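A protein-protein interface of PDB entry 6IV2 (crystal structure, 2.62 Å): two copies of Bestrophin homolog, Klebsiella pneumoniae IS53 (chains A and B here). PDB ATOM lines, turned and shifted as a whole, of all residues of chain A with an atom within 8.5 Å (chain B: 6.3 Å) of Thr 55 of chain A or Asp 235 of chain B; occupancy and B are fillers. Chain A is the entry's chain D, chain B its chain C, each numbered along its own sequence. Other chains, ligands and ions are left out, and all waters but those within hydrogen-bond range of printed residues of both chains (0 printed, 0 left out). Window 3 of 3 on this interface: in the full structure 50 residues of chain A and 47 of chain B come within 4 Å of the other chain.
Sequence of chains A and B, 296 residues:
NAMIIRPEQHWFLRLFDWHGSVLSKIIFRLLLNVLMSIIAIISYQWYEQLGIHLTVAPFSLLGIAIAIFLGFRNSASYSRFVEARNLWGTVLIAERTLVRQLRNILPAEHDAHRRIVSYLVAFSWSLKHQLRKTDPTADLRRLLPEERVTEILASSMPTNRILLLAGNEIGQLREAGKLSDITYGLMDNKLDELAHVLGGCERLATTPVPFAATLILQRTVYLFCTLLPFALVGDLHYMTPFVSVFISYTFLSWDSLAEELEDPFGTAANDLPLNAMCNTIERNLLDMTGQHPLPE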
ATOM      1  N   GLY A  51       9.419  19.743  -1.334  1.00  0.00           N
ATOM      2  CA  GLY A  51       9.652  19.014  -2.597  1.00  0.00           C
ATOM      3  C   GLY A  51      10.515  17.784  -2.338  1.00  0.00           C
ATOM      4  O   GLY A  51      10.788  17.041  -3.270  1.00  0.00           O
ATOM      5  N   ILE A  52      10.975  17.640  -1.095  1.00  0.00           N
ATOM      6  CA  ILE A  52      11.677  16.475  -0.576  1.00  0.00           C
ATOM      7  C   ILE A  52      10.635  15.463  -0.126  1.00  0.00           C
ATOM      8  O   ILE A  52       9.629  15.821   0.497  1.00  0.00           O
ATOM      9  CB  ILE A  52      12.632  16.880   0.564  1.00  0.00           C
ATOM     10  CG1 ILE A  52      11.863  17.348   1.793  1.00  0.00           C
ATOM     11  CG2 ILE A  52      13.584  17.970   0.118  1.00  0.00           C
ATOM     12  CD1 ILE A  52      11.590  16.257   2.714  1.00  0.00           C
ATOM     13  N   HIS A  53      10.836  14.200  -0.485  1.00  0.00           N
ATOM     14  CA  HIS A  53       9.909  13.159  -0.059  1.00  0.00           C
ATOM     15  C   HIS A  53      10.589  11.808  -0.187  1.00  0.00           C
ATOM     16  O   HIS A  53      11.203  11.515  -1.215  1.00  0.00           O
ATOM     17  CB  HIS A  53       8.617  13.185  -0.875  1.00  0.00           C
ATOM     18  CG  HIS A  53       7.417  12.756  -0.090  1.00  0.00           C
ATOM     19  ND1 HIS A  53       7.375  11.564   0.600  1.00  0.00           N
ATOM     20  CD2 HIS A  53       6.227  13.363   0.129  1.00  0.00           C
ATOM     21  CE1 HIS A  53       6.206  11.450   1.205  1.00  0.00           C
ATOM     22  NE2 HIS A  53       5.491  12.529   0.935  1.00  0.00           N
ATOM     23  N   LEU A  54      10.480  10.994   0.859  1.00  0.00           N
ATOM     24  CA  LEU A  54      11.232   9.754   0.970  1.00  0.00           C
ATOM     25  C   LEU A  54      10.267   8.596   1.176  1.00  0.00           C
ATOM     26  O   LEU A  54       9.375   8.668   2.026  1.00  0.00           O
ATOM     27  CB  LEU A  54      12.245   9.831   2.120  1.00  0.00           C
ATOM     28  CG  LEU A  54      13.655  10.356   1.816  1.00  0.00           C
ATOM     29  CD1 LEU A  54      13.653  11.580   0.924  1.00  0.00           C
ATOM     30  CD2 LEU A  54      14.363  10.677   3.098  1.00  0.00           C
ATOM     31  N   THR A  55      10.444   7.540   0.391  1.00  0.00           N
ATOM     32  CA  THR A  55       9.608   6.351   0.454  1.00  0.00           C
ATOM     33  C   THR A  55      10.391   5.194   1.063  1.00  0.00           C
ATOM     34  O   THR A  55      11.625   5.179   1.071  1.00  0.00           O
ATOM     35  CB  THR A  55       9.101   5.965  -0.942  1.00  0.00           C
ATOM     36  OG1 THR A  55       8.849   7.151  -1.700  1.00  0.00           O
ATOM     37  CG2 THR A  55       7.817   5.169  -0.851  1.00  0.00           C
ATOM     38  N   VAL A  56       9.650   4.219   1.587  1.00  0.00           N
ATOM     39  CA  VAL A  56      10.276   3.020   2.138  1.00  0.00           C
ATOM     40  C   VAL A  56      10.963   2.221   1.034  1.00  0.00           C
ATOM     41  O   VAL A  56      12.169   1.955   1.093  1.00  0.00           O
ATOM     42  CB  VAL A  56       9.236   2.161   2.876  1.00  0.00           C
ATOM     43  CG1 VAL A  56       9.845   0.822   3.254  1.00  0.00           C
ATOM     44  CG2 VAL A  56       8.713   2.893   4.104  1.00  0.00           C
ATOM     45  N   ALA A  57      10.201   1.842   0.008  1.00  0.00           N
ATOM     46  CA  ALA A  57      10.598   0.912  -1.043  1.00  0.00           C
ATOM     47  C   ALA A  57      11.979   1.179  -1.640  1.00  0.00           C
ATOM     48  O   ALA A  57      12.719   0.219  -1.883  1.00  0.00           O
ATOM     49  CB  ALA A  57       9.548   0.902  -2.156  1.00  0.00           C
ATOM     50  N   PRO A  58      12.370   2.432  -1.918  1.00  0.00           N
ATOM     51  CA  PRO A  58      13.762   2.645  -2.357  1.00  0.00           C
ATOM     52  C   PRO A  58      14.770   2.215  -1.311  1.00  0.00           C
ATOM     53  O   PRO A  58      15.813   1.645  -1.654  1.00  0.00           O
ATOM     54  CB  PRO A  58      13.823   4.157  -2.627  1.00  0.00           C
ATOM     55  CG  PRO A  58      12.421   4.553  -2.862  1.00  0.00           C
ATOM     56  CD  PRO A  58      11.596   3.683  -1.971  1.00  0.00           C
ATOM     57  N   PHE A  59      14.471   2.457  -0.035  1.00  0.00           N
ATOM     58  CA  PHE A  59      15.392   2.095   1.031  1.00  0.00           C
ATOM     59  C   PHE A  59      15.400   0.598   1.287  1.00  0.00           C
ATOM     60  O   PHE A  59      16.414   0.052   1.735  1.00  0.00           O
ATOM     61  CB  PHE A  59      15.036   2.851   2.310  1.00  0.00           C
ATOM     62  CG  PHE A  59      15.778   4.143   2.466  1.00  0.00           C
ATOM     63  CD1 PHE A  59      15.651   5.146   1.517  1.00  0.00           C
ATOM     64  CD2 PHE A  59      16.621   4.349   3.545  1.00  0.00           C
ATOM     65  CE1 PHE A  59      16.336   6.334   1.648  1.00  0.00           C
ATOM     66  CE2 PHE A  59      17.311   5.536   3.682  1.00  0.00           C
ATOM     67  CZ  PHE A  59      17.170   6.530   2.732  1.00  0.00           C
ATOM     68  N   SER A  60      14.285  -0.077   1.015  1.00  0.00           N
ATOM     69  CA  SER A  60      14.267  -1.532   1.102  1.00  0.00           C
ATOM     70  C   SER A  60      15.204  -2.150   0.077  1.00  0.00           C
ATOM     71  O   SER A  60      15.954  -3.081   0.391  1.00  0.00           O
ATOM     72  CB  SER A  60      12.842  -2.051   0.914  1.00  0.00           C
ATOM     73  OG  SER A  60      12.205  -2.200   2.170  1.00  0.00           O
ATOM     74  N   LEU A  61      15.162  -1.652  -1.158  1.00  0.00           N
ATOM     75  CA  LEU A  61      16.140  -2.059  -2.159  1.00  0.00           C
ATOM     76  C   LEU A  61      17.558  -1.827  -1.655  1.00  0.00           C
ATOM     77  O   LEU A  61      18.428  -2.696  -1.780  1.00  0.00           O
ATOM     78  CB  LEU A  61      15.898  -1.297  -3.460  1.00  0.00           C
ATOM     79  CG  LEU A  61      17.028  -1.412  -4.476  1.00  0.00           C
ATOM     80  CD1 LEU A  61      17.264  -2.875  -4.836  1.00  0.00           C
ATOM     81  CD2 LEU A  61      16.706  -0.598  -5.710  1.00  0.00           C
ATOM     82  N   LEU A 227      19.834   7.923   7.404  1.00  0.00           N
ATOM     83  CA  LEU A 227      18.752   8.373   6.538  1.00  0.00           C
ATOM     84  C   LEU A 227      17.542   7.461   6.596  1.00  0.00           C
ATOM     85  O   LEU A 227      16.521   7.784   5.984  1.00  0.00           O
ATOM     86  CB  LEU A 227      19.225   8.515   5.088  1.00  0.00           C
ATOM     87  CG  LEU A 227      20.468   9.386   4.899  1.00  0.00           C
ATOM     88  CD1 LEU A 227      20.969   9.257   3.473  1.00  0.00           C
ATOM     89  CD2 LEU A 227      20.200  10.847   5.269  1.00  0.00           C
ATOM     90  N   LEU A 228      17.624   6.339   7.309  1.00  0.00           N
ATOM     91  CA  LEU A 228      16.478   5.432   7.360  1.00  0.00           C
ATOM     92  C   LEU A 228      15.273   6.049   8.060  1.00  0.00           C
ATOM     93  O   LEU A 228      14.170   6.020   7.482  1.00  0.00           O
ATOM     94  CB  LEU A 228      16.888   4.107   8.006  1.00  0.00           C
ATOM     95  CG  LEU A 228      15.735   3.211   8.462  1.00  0.00           C
ATOM     96  CD1 LEU A 228      15.075   2.533   7.272  1.00  0.00           C
ATOM     97  CD2 LEU A 228      16.211   2.185   9.476  1.00  0.00           C
ATOM     98  N   PHE A 230      14.140   8.848   8.178  1.00  0.00           N
ATOM     99  CA  PHE A 230      13.464   9.782   7.289  1.00  0.00           C
ATOM    100  C   PHE A 230      12.467   9.050   6.397  1.00  0.00           C
ATOM    101  O   PHE A 230      11.278   9.380   6.371  1.00  0.00           O
ATOM    102  CB  PHE A 230      14.488  10.533   6.437  1.00  0.00           C
ATOM    103  CG  PHE A 230      15.258  11.593   7.174  1.00  0.00           C
ATOM    104  CD1 PHE A 230      15.379  11.570   8.553  1.00  0.00           C
ATOM    105  CD2 PHE A 230      15.869  12.618   6.472  1.00  0.00           C
ATOM    106  CE1 PHE A 230      16.094  12.548   9.217  1.00  0.00           C
ATOM    107  CE2 PHE A 230      16.584  13.601   7.128  1.00  0.00           C
ATOM    108  CZ  PHE A 230      16.697  13.566   8.503  1.00  0.00           C
ATOM    109  N   ALA A 231      12.941   8.037   5.668  1.00  0.00           N
ATOM    110  CA  ALA A 231      12.081   7.292   4.753  1.00  0.00           C
ATOM    111  C   ALA A 231      10.960   6.552   5.472  1.00  0.00           C
ATOM    112  O   ALA A 231       9.940   6.240   4.850  1.00  0.00           O
ATOM    113  CB  ALA A 231      12.916   6.300   3.938  1.00  0.00           C
ATOM    114  N   LEU A 232      11.122   6.270   6.764  1.00  0.00           N
ATOM    115  CA  LEU A 232      10.122   5.552   7.542  1.00  0.00           C
ATOM    116  C   LEU A 232       9.065   6.453   8.168  1.00  0.00           C
ATOM    117  O   LEU A 232       8.054   5.935   8.655  1.00  0.00           O
ATOM    118  CB  LEU A 232      10.790   4.760   8.670  1.00  0.00           C
ATOM    119  CG  LEU A 232      11.671   3.561   8.341  1.00  0.00           C
ATOM    120  CD1 LEU A 232      11.874   2.741   9.599  1.00  0.00           C
ATOM    121  CD2 LEU A 232      11.043   2.722   7.248  1.00  0.00           C
ATOM    122  N   VAL A 233       9.272   7.772   8.183  1.00  0.00           N
ATOM    123  CA  VAL A 233       8.426   8.630   9.010  1.00  0.00           C
ATOM    124  C   VAL A 233       6.998   8.680   8.480  1.00  0.00           C
ATOM    125  O   VAL A 233       6.043   8.749   9.263  1.00  0.00           O
ATOM    126  CB  VAL A 233       9.043  10.038   9.142  1.00  0.00           C
ATOM    127  CG1 VAL A 233       8.878  10.854   7.861  1.00  0.00           C
ATOM    128  CG2 VAL A 233       8.437  10.761  10.325  1.00  0.00           C
ATOM    129  N   GLY A 234       6.817   8.614   7.160  1.00  0.00           N
ATOM    130  CA  GLY A 234       5.482   8.705   6.599  1.00  0.00           C
ATOM    131  C   GLY A 234       4.597   7.517   6.908  1.00  0.00           C
ATOM    132  O   GLY A 234       3.370   7.633   6.818  1.00  0.00           O
ATOM    133  N   ASP A 235       5.188   6.380   7.273  1.00  0.00           N
ATOM    134  CA  ASP A 235       4.429   5.163   7.525  1.00  0.00           C
ATOM    135  C   ASP A 235       4.206   4.879   9.004  1.00  0.00           C
ATOM    136  O   ASP A 235       3.230   4.208   9.352  1.00  0.00           O
ATOM    137  CB  ASP A 235       5.134   3.955   6.891  1.00  0.00           C
ATOM    138  CG  ASP A 235       5.069   3.965   5.375  1.00  0.00           C
ATOM    139  OD1 ASP A 235       4.756   5.027   4.796  1.00  0.00           O
ATOM    140  OD2 ASP A 235       5.327   2.910   4.759  1.00  0.00           O
ATOM    141  N   TYR B  44      10.493  15.100 -15.615  1.00  0.00           N
ATOM    142  CA  TYR B  44       9.254  14.713 -14.953  1.00  0.00           C
ATOM    143  C   TYR B  44       8.076  15.581 -15.362  1.00  0.00           C
ATOM    144  O   TYR B  44       6.933  15.131 -15.249  1.00  0.00           O
ATOM    145  CB  TYR B  44       9.414  14.774 -13.435  1.00  0.00           C
ATOM    146  CG  TYR B  44       8.323  14.038 -12.692  1.00  0.00           C
ATOM    147  CD1 TYR B  44       7.833  12.832 -13.168  1.00  0.00           C
ATOM    148  CD2 TYR B  44       7.785  14.547 -11.519  1.00  0.00           C
ATOM    149  CE1 TYR B  44       6.841  12.149 -12.498  1.00  0.00           C
ATOM    150  CE2 TYR B  44       6.790  13.872 -10.840  1.00  0.00           C
ATOM    151  CZ  TYR B  44       6.322  12.673 -11.334  1.00  0.00           C
ATOM    152  OH  TYR B  44       5.333  11.991 -10.665  1.00  0.00           O
ATOM    153  N   VAL B  56       8.266   2.097  -9.170  1.00  0.00           N
ATOM    154  CA  VAL B  56       9.474   1.673  -8.461  1.00  0.00           C
ATOM    155  C   VAL B  56       9.562   0.154  -8.343  1.00  0.00           C
ATOM    156  O   VAL B  56      10.643  -0.422  -8.504  1.00  0.00           O
ATOM    157  CB  VAL B  56       9.530   2.356  -7.076  1.00  0.00           C
ATOM    158  CG1 VAL B  56      10.453   1.605  -6.128  1.00  0.00           C
ATOM    159  CG2 VAL B  56       9.960   3.817  -7.203  1.00  0.00           C
ATOM    160  N   ALA B 231      12.616   6.102 -12.489  1.00  0.00           N
ATOM    161  CA  ALA B 231      11.590   5.413 -11.721  1.00  0.00           C
ATOM    162  C   ALA B 231      11.520   5.918 -10.290  1.00  0.00           C
ATOM    163  O   ALA B 231      10.500   5.716  -9.624  1.00  0.00           O
ATOM    164  CB  ALA B 231      11.840   3.903 -11.728  1.00  0.00           C
ATOM    165  N   LEU B 232      12.581   6.567  -9.807  1.00  0.00           N
ATOM    166  CA  LEU B 232      12.553   7.174  -8.485  1.00  0.00           C
ATOM    167  C   LEU B 232      11.932   8.565  -8.508  1.00  0.00           C
ATOM    168  O   LEU B 232      11.277   8.958  -7.535  1.00  0.00           O
ATOM    169  CB  LEU B 232      13.970   7.255  -7.910  1.00  0.00           C
ATOM    170  CG  LEU B 232      14.678   5.969  -7.470  1.00  0.00           C
ATOM    171  CD1 LEU B 232      16.047   6.316  -6.900  1.00  0.00           C
ATOM    172  CD2 LEU B 232      13.854   5.188  -6.454  1.00  0.00           C
ATOM    173  N   VAL B 233      11.981   9.231  -9.670  1.00  0.00           N
ATOM    174  CA  VAL B 233      11.567  10.665  -9.802  1.00  0.00           C
ATOM    175  C   VAL B 233      10.183  10.765  -9.221  1.00  0.00           C
ATOM    176  O   VAL B 233       9.929  11.681  -8.502  1.00  0.00           O
ATOM    177  CB  VAL B 233      11.545  11.147 -11.255  1.00  0.00           C
ATOM    178  CG1 VAL B 233      12.138  12.535 -11.406  1.00  0.00           C
ATOM    179  CG2 VAL B 233      12.240  10.160 -12.162  1.00  0.00           C
ATOM    180  N   GLY B 234       9.449   9.684  -9.390  1.00  0.00           N
ATOM    181  CA  GLY B 234       8.038   9.515  -9.031  1.00  0.00           C
ATOM    182  C   GLY B 234       7.700   9.699  -7.574  1.00  0.00           C
ATOM    183  O   GLY B 234       6.568  10.020  -7.343  1.00  0.00           O
ATOM    184  N   ASP B 235       8.606   9.448  -6.650  1.00  0.00           N
ATOM    185  CA  ASP B 235       8.187   9.736  -5.264  1.00  0.00           C
ATOM    186  C   ASP B 235       9.299  10.473  -4.547  1.00  0.00           C
ATOM    187  O   ASP B 235       9.104  10.827  -3.407  1.00  0.00           O
ATOM    188  CB  ASP B 235       7.794   8.476  -4.511  1.00  0.00           C
ATOM    189  CG  ASP B 235       8.137   7.247  -5.306  1.00  0.00           C
ATOM    190  OD1 ASP B 235       8.887   7.406  -6.262  1.00  0.00           O
ATOM    191  OD2 ASP B 235       7.628   6.181  -4.980  1.00  0.00           O
ATOM    192  N   LEU B 236      10.401  10.699  -5.223  1.00  0.00           N
ATOM    193  CA  LEU B 236      11.462  11.373  -4.461  1.00  0.00           C
ATOM    194  C   LEU B 236      11.606  12.826  -4.897  1.00  0.00           C
ATOM    195  O   LEU B 236      12.158  13.599  -4.121  1.00  0.00           O
ATOM    196  CB  LEU B 236      12.717  10.532  -4.626  1.00  0.00           C
ATOM    197  CG  LEU B 236      12.502   9.114  -4.111  1.00  0.00           C
ATOM    198  CD1 LEU B 236      13.780   8.316  -4.164  1.00  0.00           C
ATOM    199  CD2 LEU B 236      11.934   9.126  -2.705  1.00  0.00           C
ATOM    200  N   HIS B 237      11.133  13.138  -6.096  1.00  0.00           N
ATOM    201  CA  HIS B 237      11.146  14.540  -6.554  1.00  0.00           C
ATOM    202  C   HIS B 237      12.584  15.036  -6.493  1.00  0.00           C
ATOM    203  O   HIS B 237      13.386  14.586  -7.268  1.00  0.00           O
ATOM    204  CB  HIS B 237      10.121  15.333  -5.746  1.00  0.00           C
ATOM    205  CG  HIS B 237       8.723  15.252  -6.279  1.00  0.00           C
ATOM    206  ND1 HIS B 237       7.798  14.353  -5.795  1.00  0.00           N
ATOM    207  CD2 HIS B 237       8.088  15.970  -7.227  1.00  0.00           C
ATOM    208  CE1 HIS B 237       6.662  14.520  -6.422  1.00  0.00           C
ATOM    209  NE2 HIS B 237       6.815  15.501  -7.299  1.00  0.00           N
ATOM    210  N   THR B 240      15.231  12.681  -5.034  1.00  0.00           N
ATOM    211  CA  THR B 240      15.567  11.631  -5.983  1.00  0.00           C
ATOM    212  C   THR B 240      17.079  11.516  -6.141  1.00  0.00           C
ATOM    213  O   THR B 240      17.618  10.419  -5.960  1.00  0.00           O
ATOM    214  CB  THR B 240      14.902  11.885  -7.338  1.00  0.00           C
ATOM    215  OG1 THR B 240      13.533  11.478  -7.271  1.00  0.00           O
ATOM    216  CG2 THR B 240      15.613  11.122  -8.457  1.00  0.00           C
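Hydrophobic or aromatic side chains of chain B that line the printed part of chain A: Leu 232, Leu 236 and His 237. Of the 19 printed residues of chain A, 5 touch a printed residue of chain B. Among the printed residues, 8 pairs touch across the chains.
The backbone carbonyl oxygen of Leu 232 of chain B is in hydrogen-bond range of the side-chain hydroxyl of Thr 240 of chain B, 3.4 Å away. The backbone carbonyl oxygen (O) of His 237 of chain B lies close to the side-chain hydroxyl (OG1) of Thr 240 of chain B, 3.1 Å away.
Positions printed for both chains: 56, 231, 232, 233, 234 and 235. Of the 8 pairs that touch across the chains among the printed residues, none has its exchanged pair printed and touching as well.
The backbone carbonyl oxygen (O) of Asp 235 of chain B sits close to the backbone carbonyl oxygen (O) of His 53 of chain A.
Thr 55 of chain A touches just these residues of chain B: Asp 235 and Leu 236. Asp 235 of chain B touches just these residues of chain A: His 53 (3.1 Å) and Thr 55 (3.3 Å). Printed residues of chain A within 4 Å of Leu 236 of chain B: Gly 51 (3.8 Å), His 53 (2.9 Å), Leu 54 (3.8 Å) and Thr 55 (3.8 Å). Of the printed residues of chain A, Leu 232 of chain B touches Pro 58 (3.9 Å). Val 56 of chain B touches none of the printed residues of chain A. The nearest printed residue of chain B that does not touch Thr 55 of chain A is Gly 234 of chain B (6.5 Å).
Gly 51 of chain A touches Leu 236 of chain B. CB of His 237 of chain B touches O of Gly 51 of chain A (3.1 Å). O of His 53 of chain A touches CD2 of Leu 236 of chain B, at 2.9 Å. CA of Leu 54 of chain A touches CD2 of Leu 236 of chain B, 3.8 Å away. CB of Asp 235 of chain B touches OG1 of Thr 55 of chain A (3.3 Å). N of Thr 55 of chain A touches CD2 of Leu 236 of chain B (3.8 Å). CD2 of Leu 232 of chain B touches CG of Pro 58 of chain A, at 3.9 Å.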
